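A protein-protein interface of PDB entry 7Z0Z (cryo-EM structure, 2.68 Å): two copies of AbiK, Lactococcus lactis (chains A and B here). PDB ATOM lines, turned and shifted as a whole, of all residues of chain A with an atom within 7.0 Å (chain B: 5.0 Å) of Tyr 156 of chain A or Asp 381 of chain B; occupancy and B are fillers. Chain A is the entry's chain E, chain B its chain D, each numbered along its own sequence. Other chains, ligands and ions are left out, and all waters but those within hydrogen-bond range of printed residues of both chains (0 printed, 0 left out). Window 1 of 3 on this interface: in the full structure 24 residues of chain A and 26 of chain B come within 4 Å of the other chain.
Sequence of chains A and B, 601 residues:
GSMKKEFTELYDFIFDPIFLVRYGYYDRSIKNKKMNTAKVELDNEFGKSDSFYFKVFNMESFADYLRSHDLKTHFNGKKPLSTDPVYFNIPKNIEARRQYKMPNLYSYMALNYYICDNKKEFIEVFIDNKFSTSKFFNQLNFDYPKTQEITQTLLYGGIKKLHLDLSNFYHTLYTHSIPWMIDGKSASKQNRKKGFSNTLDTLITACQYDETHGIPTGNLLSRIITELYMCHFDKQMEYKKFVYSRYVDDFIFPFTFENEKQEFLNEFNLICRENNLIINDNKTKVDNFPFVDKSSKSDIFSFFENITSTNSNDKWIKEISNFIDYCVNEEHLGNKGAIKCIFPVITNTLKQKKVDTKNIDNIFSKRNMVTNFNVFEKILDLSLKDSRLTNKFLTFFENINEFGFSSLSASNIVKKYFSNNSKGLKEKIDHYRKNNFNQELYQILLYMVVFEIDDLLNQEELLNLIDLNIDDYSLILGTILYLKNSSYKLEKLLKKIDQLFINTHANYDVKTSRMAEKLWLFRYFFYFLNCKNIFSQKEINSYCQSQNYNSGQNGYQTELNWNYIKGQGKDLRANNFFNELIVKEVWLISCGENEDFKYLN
Among the printed residues, pairs that only touch across the chains: Ile 159 of chain A with Lys 385 of chain B, Gln 152 of chain A with Phe 373 of chain B, Tyr 156 of chain A with Asp 381 of chain B, Tyr 156 of chain A with Glu 377 of chain B, Tyr 156 of chain A with Asn 374 of chain B, Tyr 156 of chain A with Phe 373 of chain B, Thr 153 of chain A with Phe 373 of chain B, Phe 289 of chain A with Leu 382 of chain B, Glu 149 of chain A with Phe 373 of chain B, Gly 157 of chain A with Tyr 417 of chain B, Phe 289 of chain A with Lys 385 of chain B, Tyr 156 of chain A with Tyr 417 of chain B and Leu 155 of chain A with Lys 385 of chain B.
No position is printed for both chains. Of the 17 pairs that touch across the chains among the printed residues, none has its exchanged pair printed and touching as well.
Printed residues of chain B within 4 Å of Gln 152 of chain A: Phe 373 (3.2 Å) and Lys 378 (3.4 Å). Tyr 156 of chain A touches just these residues of chain B: Phe 373 (3.6 Å), Asn 374 (3.6 Å), Glu 377 (3.4 Å), Lys 378 (3.2 Å), Asp 381 (3.2 Å) and Tyr 417 (3.96 Å). Of the printed residues of chain B, Phe 289 of chain A touches Leu 382 (3.7 Å) and Lys 385 (3.8 Å). Printed residues of chain A within 4 Å of Asn 374 of chain B: Tyr 156. Printed residues of chain A within 4 Å of Lys 378 of chain B: Gln 152 (3.4 Å) and Tyr 156 (3.2 Å). Asp 381 of chain B touches just these residues of chain A: Tyr 156 (3.2 Å) and Gly 157 (2.7 Å). The nearest residue of chain B that does not touch Tyr 156 of chain A is Asn 421 of chain B (4.2 Å). The nearest residue of chain A that does not touch Asp 381 of chain B is Leu 155 of chain A (4.3 Å).
Of the 14 printed residues of chain A, 9 touch a printed residue of chain B. Printed residues of chain B that touch a printed residue of chain A: Phe 373, Asn 374, Glu 377, Lys 378, Asp 381, Leu 382, Lys 385 and Tyr 417. Hydrophobic or aromatic side chains of chain B that line the printed part of chain A: Phe 373, Leu 382 and Tyr 417.
The side-chain amino group (NZ) of Lys 385 of chain B sits close to the backbone carbonyl oxygen (O) of Gly 158 of chain A, at 2.4 Å. OH of Tyr 156 of chain A lies close to N of Lys 378 of chain B (3.2 Å). The side-chain amide nitrogen (NE2) of Gln 152 of chain A lies close to the side-chain amino group (NZ) of Lys 378 of chain B (3.4 Å). The side-chain carboxylate of Asp 381 of chain B lies within hydrogen-bond range of the backbone NH of Gly 157 of chain A, 2.7 Å away.
N of Ile 159 of chain A lies within hydrogen-bond range of O of Phe 255 of chain A, 3.3 Å away. NZ of Lys 385 of chain B is in salt-bridge range of OD2 of Asp 381 of chain B, at 3.4 Å. The side-chain amide nitrogen (ND2) of Asn 421 of chain B lies within hydrogen-bond range of the backbone carbonyl oxygen (O) of Tyr 417 of chain B (3.0 Å). O of Glu 149 of chain A is in hydrogen-bond range of OG1 of Thr 153 of chain A (2.8 Å). The side-chain amide oxygen (OD1) of Asn 374 of chain B sits at hydrogen-bond distance from the backbone NH (N) of Glu 377 of chain B. N of Phe 289 of chain A is in hydrogen-bond range of O of Ile 159 of chain A, at 3.2 Å.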
ATOM      1  N   GLU A 149      15.848 -17.164  29.345  1.00  0.00           N
ATOM      2  CA  GLU A 149      15.671 -17.418  27.919  1.00  0.00           C
ATOM      3  C   GLU A 149      14.474 -18.322  27.667  1.00  0.00           C
ATOM      4  O   GLU A 149      13.714 -18.111  26.712  1.00  0.00           O
ATOM      5  CB  GLU A 149      16.927 -18.049  27.330  1.00  0.00           C
ATOM      6  CG  GLU A 149      18.152 -17.175  27.352  1.00  0.00           C
ATOM      7  CD  GLU A 149      19.362 -17.883  26.784  1.00  0.00           C
ATOM      8  OE1 GLU A 149      19.208 -18.594  25.770  1.00  0.00           O
ATOM      9  OE2 GLU A 149      20.465 -17.735  27.351  1.00  0.00           O
ATOM     10  N   THR A 151      11.808 -18.581  29.550  1.00  0.00           N
ATOM     11  CA  THR A 151      10.624 -17.756  29.769  1.00  0.00           C
ATOM     12  C   THR A 151      10.348 -16.864  28.567  1.00  0.00           C
ATOM     13  O   THR A 151       9.204 -16.750  28.110  1.00  0.00           O
ATOM     14  CB  THR A 151      10.804 -16.913  31.029  1.00  0.00           C
ATOM     15  OG1 THR A 151      10.680 -17.747  32.183  1.00  0.00           O
ATOM     16  CG2 THR A 151       9.752 -15.831  31.101  1.00  0.00           C
ATOM     17  N   GLN A 152      11.394 -16.228  28.037  1.00  0.00           N
ATOM     18  CA  GLN A 152      11.239 -15.386  26.857  1.00  0.00           C
ATOM     19  C   GLN A 152      10.634 -16.170  25.705  1.00  0.00           C
ATOM     20  O   GLN A 152       9.682 -15.717  25.064  1.00  0.00           O
ATOM     21  CB  GLN A 152      12.591 -14.800  26.452  1.00  0.00           C
ATOM     22  CG  GLN A 152      13.159 -13.818  27.454  1.00  0.00           C
ATOM     23  CD  GLN A 152      14.508 -13.274  27.036  1.00  0.00           C
ATOM     24  OE1 GLN A 152      15.063 -13.680  26.018  1.00  0.00           O
ATOM     25  NE2 GLN A 152      15.044 -12.354  27.827  1.00  0.00           N
ATOM     26  N   THR A 153      11.165 -17.363  25.441  1.00  0.00           N
ATOM     27  CA  THR A 153      10.646 -18.172  24.347  1.00  0.00           C
ATOM     28  C   THR A 153       9.195 -18.571  24.586  1.00  0.00           C
ATOM     29  O   THR A 153       8.408 -18.677  23.640  1.00  0.00           O
ATOM     30  CB  THR A 153      11.516 -19.409  24.156  1.00  0.00           C
ATOM     31  OG1 THR A 153      12.895 -19.034  24.237  1.00  0.00           O
ATOM     32  CG2 THR A 153      11.252 -20.032  22.804  1.00  0.00           C
ATOM     33  N   LEU A 154       8.822 -18.808  25.845  1.00  0.00           N
ATOM     34  CA  LEU A 154       7.444 -19.184  26.140  1.00  0.00           C
ATOM     35  C   LEU A 154       6.481 -18.009  26.044  1.00  0.00           C
ATOM     36  O   LEU A 154       5.281 -18.224  25.860  1.00  0.00           O
ATOM     37  CB  LEU A 154       7.341 -19.802  27.533  1.00  0.00           C
ATOM     38  CG  LEU A 154       7.753 -21.265  27.665  1.00  0.00           C
ATOM     39  CD1 LEU A 154       8.276 -21.538  29.059  1.00  0.00           C
ATOM     40  CD2 LEU A 154       6.592 -22.171  27.340  1.00  0.00           C
ATOM     41  N   LEU A 155       6.973 -16.781  26.163  1.00  0.00           N
ATOM     42  CA  LEU A 155       6.118 -15.604  26.199  1.00  0.00           C
ATOM     43  C   LEU A 155       5.855 -15.017  24.818  1.00  0.00           C
ATOM     44  O   LEU A 155       5.267 -13.937  24.718  1.00  0.00           O
ATOM     45  CB  LEU A 155       6.738 -14.546  27.110  1.00  0.00           C
ATOM     46  CG  LEU A 155       6.693 -14.864  28.603  1.00  0.00           C
ATOM     47  CD1 LEU A 155       6.891 -13.617  29.427  1.00  0.00           C
ATOM     48  CD2 LEU A 155       5.389 -15.543  28.971  1.00  0.00           C
ATOM     49  N   TYR A 156       6.276 -15.702  23.761  1.00  0.00           N
ATOM     50  CA  TYR A 156       6.104 -15.202  22.405  1.00  0.00           C
ATOM     51  C   TYR A 156       4.629 -15.116  22.036  1.00  0.00           C
ATOM     52  O   TYR A 156       3.808 -15.933  22.460  1.00  0.00           O
ATOM     53  CB  TYR A 156       6.830 -16.118  21.423  1.00  0.00           C
ATOM     54  CG  TYR A 156       8.317 -15.887  21.351  1.00  0.00           C
ATOM     55  CD1 TYR A 156       8.935 -14.956  22.168  1.00  0.00           C
ATOM     56  CD2 TYR A 156       9.113 -16.651  20.517  1.00  0.00           C
ATOM     57  CE1 TYR A 156      10.291 -14.758  22.117  1.00  0.00           C
ATOM     58  CE2 TYR A 156      10.469 -16.463  20.467  1.00  0.00           C
ATOM     59  CZ  TYR A 156      11.053 -15.518  21.271  1.00  0.00           C
ATOM     60  OH  TYR A 156      12.409 -15.329  21.225  1.00  0.00           O
ATOM     61  N   GLY A 157       4.294 -14.110  21.233  1.00  0.00           N
ATOM     62  CA  GLY A 157       2.970 -13.981  20.669  1.00  0.00           C
ATOM     63  C   GLY A 157       1.954 -13.262  21.524  1.00  0.00           C
ATOM     64  O   GLY A 157       0.797 -13.141  21.104  1.00  0.00           O
ATOM     65  N   GLY A 158       2.331 -12.780  22.699  1.00  0.00           N
ATOM     66  CA  GLY A 158       1.365 -12.153  23.572  1.00  0.00           C
ATOM     67  C   GLY A 158       1.574 -10.668  23.756  1.00  0.00           C
ATOM     68  O   GLY A 158       2.642 -10.234  24.192  1.00  0.00           O
ATOM     69  N   ILE A 159       0.552  -9.874  23.427  1.00  0.00           N
ATOM     70  CA  ILE A 159       0.619  -8.431  23.635  1.00  0.00           C
ATOM     71  C   ILE A 159       0.334  -8.063  25.080  1.00  0.00           C
ATOM     72  O   ILE A 159       0.518  -6.905  25.472  1.00  0.00           O
ATOM     73  CB  ILE A 159      -0.367  -7.725  22.684  1.00  0.00           C
ATOM     74  CG1 ILE A 159      -0.068  -6.236  22.594  1.00  0.00           C
ATOM     75  CG2 ILE A 159      -1.786  -7.888  23.172  1.00  0.00           C
ATOM     76  CD1 ILE A 159       1.253  -5.944  21.969  1.00  0.00           C
ATOM     77  N   VAL A 243      -0.677 -22.093  27.099  1.00  0.00           N
ATOM     78  CA  VAL A 243       0.766 -21.887  27.116  1.00  0.00           C
ATOM     79  C   VAL A 243       1.078 -20.802  28.130  1.00  0.00           C
ATOM     80  O   VAL A 243       0.441 -19.743  28.127  1.00  0.00           O
ATOM     81  CB  VAL A 243       1.314 -21.503  25.729  1.00  0.00           C
ATOM     82  CG1 VAL A 243       2.795 -21.196  25.812  1.00  0.00           C
ATOM     83  CG2 VAL A 243       1.064 -22.613  24.732  1.00  0.00           C
ATOM     84  N   PRO A 254       0.917 -15.356  28.619  1.00  0.00           N
ATOM     85  CA  PRO A 254       0.835 -14.381  27.530  1.00  0.00           C
ATOM     86  C   PRO A 254      -0.461 -14.548  26.752  1.00  0.00           C
ATOM     87  O   PRO A 254      -0.867 -15.663  26.422  1.00  0.00           O
ATOM     88  CB  PRO A 254       2.052 -14.719  26.666  1.00  0.00           C
ATOM     89  CG  PRO A 254       2.235 -16.173  26.870  1.00  0.00           C
ATOM     90  CD  PRO A 254       1.804 -16.482  28.280  1.00  0.00           C
ATOM     91  N   PHE A 255      -1.110 -13.428  26.460  1.00  0.00           N
ATOM     92  CA  PHE A 255      -2.370 -13.461  25.738  1.00  0.00           C
ATOM     93  C   PHE A 255      -2.540 -12.148  24.993  1.00  0.00           C
ATOM     94  O   PHE A 255      -1.861 -11.160  25.273  1.00  0.00           O
ATOM     95  CB  PHE A 255      -3.547 -13.734  26.686  1.00  0.00           C
ATOM     96  CG  PHE A 255      -3.887 -12.584  27.589  1.00  0.00           C
ATOM     97  CD1 PHE A 255      -3.226 -12.416  28.788  1.00  0.00           C
ATOM     98  CD2 PHE A 255      -4.842 -11.656  27.224  1.00  0.00           C
ATOM     99  CE1 PHE A 255      -3.523 -11.360  29.609  1.00  0.00           C
ATOM    100  CE2 PHE A 255      -5.145 -10.603  28.046  1.00  0.00           C
ATOM    101  CZ  PHE A 255      -4.481 -10.452  29.239  1.00  0.00           C
ATOM    102  N   PHE A 289       1.710  -4.230  26.821  1.00  0.00           N
ATOM    103  CA  PHE A 289       2.879  -3.838  26.055  1.00  0.00           C
ATOM    104  C   PHE A 289       2.806  -2.348  25.726  1.00  0.00           C
ATOM    105  O   PHE A 289       1.735  -1.838  25.388  1.00  0.00           O
ATOM    106  CB  PHE A 289       2.975  -4.678  24.782  1.00  0.00           C
ATOM    107  CG  PHE A 289       4.162  -4.365  23.924  1.00  0.00           C
ATOM    108  CD1 PHE A 289       4.101  -3.378  22.959  1.00  0.00           C
ATOM    109  CD2 PHE A 289       5.346  -5.048  24.097  1.00  0.00           C
ATOM    110  CE1 PHE A 289       5.191  -3.097  22.174  1.00  0.00           C
ATOM    111  CE2 PHE A 289       6.442  -4.766  23.315  1.00  0.00           C
ATOM    112  CZ  PHE A 289       6.363  -3.789  22.354  1.00  0.00           C
ATOM    113  N   PHE B 373      16.000 -20.966  22.150  1.00  0.00           N
ATOM    114  CA  PHE B 373      15.901 -19.519  22.013  1.00  0.00           C
ATOM    115  C   PHE B 373      16.719 -19.047  20.823  1.00  0.00           C
ATOM    116  O   PHE B 373      17.901 -19.383  20.703  1.00  0.00           O
ATOM    117  CB  PHE B 373      16.381 -18.824  23.288  1.00  0.00           C
ATOM    118  CG  PHE B 373      16.480 -17.331  23.167  1.00  0.00           C
ATOM    119  CD1 PHE B 373      15.358 -16.537  23.280  1.00  0.00           C
ATOM    120  CD2 PHE B 373      17.702 -16.725  22.953  1.00  0.00           C
ATOM    121  CE1 PHE B 373      15.452 -15.173  23.176  1.00  0.00           C
ATOM    122  CE2 PHE B 373      17.799 -15.359  22.846  1.00  0.00           C
ATOM    123  CZ  PHE B 373      16.674 -14.584  22.957  1.00  0.00           C
ATOM    124  N   ASN B 374      16.093 -18.265  19.950  1.00  0.00           N
ATOM    125  CA  ASN B 374      16.782 -17.613  18.849  1.00  0.00           C
ATOM    126  C   ASN B 374      16.487 -16.123  18.929  1.00  0.00           C
ATOM    127  O   ASN B 374      15.342 -15.723  19.148  1.00  0.00           O
ATOM    128  CB  ASN B 374      16.339 -18.195  17.504  1.00  0.00           C
ATOM    129  CG  ASN B 374      17.051 -17.568  16.335  1.00  0.00           C
ATOM    130  OD1 ASN B 374      16.893 -16.388  16.051  1.00  0.00           O
ATOM    131  ND2 ASN B 374      17.850 -18.364  15.647  1.00  0.00           N
ATOM    132  N   GLU B 377      14.137 -14.646  16.286  1.00  0.00           N
ATOM    133  CA  GLU B 377      12.744 -14.940  16.600  1.00  0.00           C
ATOM    134  C   GLU B 377      12.197 -13.975  17.643  1.00  0.00           C
ATOM    135  O   GLU B 377      11.028 -13.579  17.580  1.00  0.00           O
ATOM    136  CB  GLU B 377      12.619 -16.380  17.086  1.00  0.00           C
ATOM    137  CG  GLU B 377      11.307 -17.038  16.749  1.00  0.00           C
ATOM    138  CD  GLU B 377      11.066 -18.282  17.570  1.00  0.00           C
ATOM    139  OE1 GLU B 377      11.971 -18.664  18.341  1.00  0.00           O
ATOM    140  OE2 GLU B 377       9.979 -18.882  17.447  1.00  0.00           O
ATOM    141  N   LYS B 378      13.025 -13.586  18.612  1.00  0.00           N
ATOM    142  CA  LYS B 378      12.593 -12.596  19.590  1.00  0.00           C
ATOM    143  C   LYS B 378      12.326 -11.254  18.931  1.00  0.00           C
ATOM    144  O   LYS B 378      11.343 -10.574  19.254  1.00  0.00           O
ATOM    145  CB  LYS B 378      13.640 -12.445  20.688  1.00  0.00           C
ATOM    146  CG  LYS B 378      13.203 -11.509  21.792  1.00  0.00           C
ATOM    147  CD  LYS B 378      14.215 -11.433  22.904  1.00  0.00           C
ATOM    148  CE  LYS B 378      13.741 -10.485  23.979  1.00  0.00           C
ATOM    149  NZ  LYS B 378      14.718 -10.388  25.087  1.00  0.00           N
ATOM    150  N   ILE B 379      13.192 -10.851  18.001  1.00  0.00           N
ATOM    151  CA  ILE B 379      12.992  -9.582  17.310  1.00  0.00           C
ATOM    152  C   ILE B 379      11.743  -9.642  16.436  1.00  0.00           C
ATOM    153  O   ILE B 379      10.987  -8.670  16.336  1.00  0.00           O
ATOM    154  CB  ILE B 379      14.251  -9.223  16.503  1.00  0.00           C
ATOM    155  CG1 ILE B 379      15.404  -8.904  17.448  1.00  0.00           C
ATOM    156  CG2 ILE B 379      14.005  -8.026  15.627  1.00  0.00           C
ATOM    157  CD1 ILE B 379      16.764  -9.068  16.828  1.00  0.00           C
ATOM    158  N   LEU B 380      11.495 -10.793  15.809  1.00  0.00           N
ATOM    159  CA  LEU B 380      10.291 -10.967  15.003  1.00  0.00           C
ATOM    160  C   LEU B 380       9.031 -10.892  15.856  1.00  0.00           C
ATOM    161  O   LEU B 380       8.039 -10.267  15.462  1.00  0.00           O
ATOM    162  CB  LEU B 380      10.364 -12.297  14.260  1.00  0.00           C
ATOM    163  CG  LEU B 380       9.079 -12.886  13.689  1.00  0.00           C
ATOM    164  CD1 LEU B 380       8.717 -12.204  12.395  1.00  0.00           C
ATOM    165  CD2 LEU B 380       9.259 -14.370  13.471  1.00  0.00           C
ATOM    166  N   ASP B 381       9.047 -11.526  17.028  1.00  0.00           N
ATOM    167  CA  ASP B 381       7.904 -11.441  17.930  1.00  0.00           C
ATOM    168  C   ASP B 381       7.670 -10.009  18.389  1.00  0.00           C
ATOM    169  O   ASP B 381       6.525  -9.538  18.429  1.00  0.00           O
ATOM    170  CB  ASP B 381       8.122 -12.362  19.126  1.00  0.00           C
ATOM    171  CG  ASP B 381       6.849 -12.622  19.894  1.00  0.00           C
ATOM    172  OD1 ASP B 381       5.890 -13.140  19.292  1.00  0.00           O
ATOM    173  OD2 ASP B 381       6.808 -12.317  21.101  1.00  0.00           O
ATOM    174  N   LEU B 382       8.745  -9.299  18.732  1.00  0.00           N
ATOM    175  CA  LEU B 382       8.620  -7.889  19.074  1.00  0.00           C
ATOM    176  C   LEU B 382       7.969  -7.103  17.946  1.00  0.00           C
ATOM    177  O   LEU B 382       7.090  -6.270  18.186  1.00  0.00           O
ATOM    178  CB  LEU B 382       9.990  -7.304  19.390  1.00  0.00           C
ATOM    179  CG  LEU B 382       9.955  -5.835  19.788  1.00  0.00           C
ATOM    180  CD1 LEU B 382       9.257  -5.654  21.117  1.00  0.00           C
ATOM    181  CD2 LEU B 382      11.352  -5.290  19.826  1.00  0.00           C
ATOM    182  N   SER B 383       8.399  -7.348  16.708  1.00  0.00           N
ATOM    183  CA  SER B 383       7.803  -6.654  15.575  1.00  0.00           C
ATOM    184  C   SER B 383       6.321  -6.969  15.458  1.00  0.00           C
ATOM    185  O   SER B 383       5.516  -6.091  15.132  1.00  0.00           O
ATOM    186  CB  SER B 383       8.525  -7.038  14.292  1.00  0.00           C
ATOM    187  OG  SER B 383       8.134  -8.333  13.882  1.00  0.00           O
ATOM    188  N   LEU B 384       5.938  -8.219  15.714  1.00  0.00           N
ATOM    189  CA  LEU B 384       4.530  -8.587  15.624  1.00  0.00           C
ATOM    190  C   LEU B 384       3.697  -8.019  16.764  1.00  0.00           C
ATOM    191  O   LEU B 384       2.472  -7.947  16.637  1.00  0.00           O
ATOM    192  CB  LEU B 384       4.376 -10.104  15.575  1.00  0.00           C
ATOM    193  CG  LEU B 384       4.901 -10.767  14.305  1.00  0.00           C
ATOM    194  CD1 LEU B 384       5.269 -12.202  14.566  1.00  0.00           C
ATOM    195  CD2 LEU B 384       3.858 -10.689  13.215  1.00  0.00           C
ATOM    196  N   LYS B 385       4.318  -7.615  17.873  1.00  0.00           N
ATOM    197  CA  LYS B 385       3.524  -7.051  18.963  1.00  0.00           C
ATOM    198  C   LYS B 385       2.960  -5.681  18.600  1.00  0.00           C
ATOM    199  O   LYS B 385       1.858  -5.328  19.032  1.00  0.00           O
ATOM    200  CB  LYS B 385       4.349  -6.975  20.243  1.00  0.00           C
ATOM    201  CG  LYS B 385       4.697  -8.338  20.790  1.00  0.00           C
ATOM    202  CD  LYS B 385       5.462  -8.255  22.081  1.00  0.00           C
ATOM    203  CE  LYS B 385       5.854  -9.635  22.535  1.00  0.00           C
ATOM    204  NZ  LYS B 385       4.668 -10.430  22.921  1.00  0.00           N
ATOM    205  N   TYR B 417       8.603 -20.095  13.606  1.00  0.00           N
ATOM    206  CA  TYR B 417       7.758 -19.258  14.452  1.00  0.00           C
ATOM    207  C   TYR B 417       6.299 -19.343  14.028  1.00  0.00           C
ATOM    208  O   TYR B 417       5.406 -19.504  14.867  1.00  0.00           O
ATOM    209  CB  TYR B 417       8.244 -17.809  14.422  1.00  0.00           C
ATOM    210  CG  TYR B 417       7.417 -16.853  15.262  1.00  0.00           C
ATOM    211  CD1 TYR B 417       6.203 -16.362  14.802  1.00  0.00           C
ATOM    212  CD2 TYR B 417       7.843 -16.455  16.516  1.00  0.00           C
ATOM    213  CE1 TYR B 417       5.450 -15.508  15.556  1.00  0.00           C
ATOM    214  CE2 TYR B 417       7.089 -15.595  17.278  1.00  0.00           C
ATOM    215  CZ  TYR B 417       5.894 -15.124  16.793  1.00  0.00           C
ATOM    216  OH  TYR B 417       5.135 -14.265  17.548  1.00  0.00           O
ATOM    217  N   ASN B 421       3.188 -20.893  16.247  1.00  0.00           N
ATOM    218  CA  ASN B 421       2.134 -19.992  16.691  1.00  0.00           C
ATOM    219  C   ASN B 421       0.979 -19.934  15.699  1.00  0.00           C
ATOM    220  O   ASN B 421       0.281 -18.925  15.616  1.00  0.00           O
ATOM    221  CB  ASN B 421       2.706 -18.596  16.924  1.00  0.00           C
ATOM    222  CG  ASN B 421       3.738 -18.571  18.027  1.00  0.00           C
ATOM    223  OD1 ASN B 421       3.401 -18.578  19.208  1.00  0.00           O
ATOM    224  ND2 ASN B 421       5.005 -18.566  17.648  1.00  0.00           N
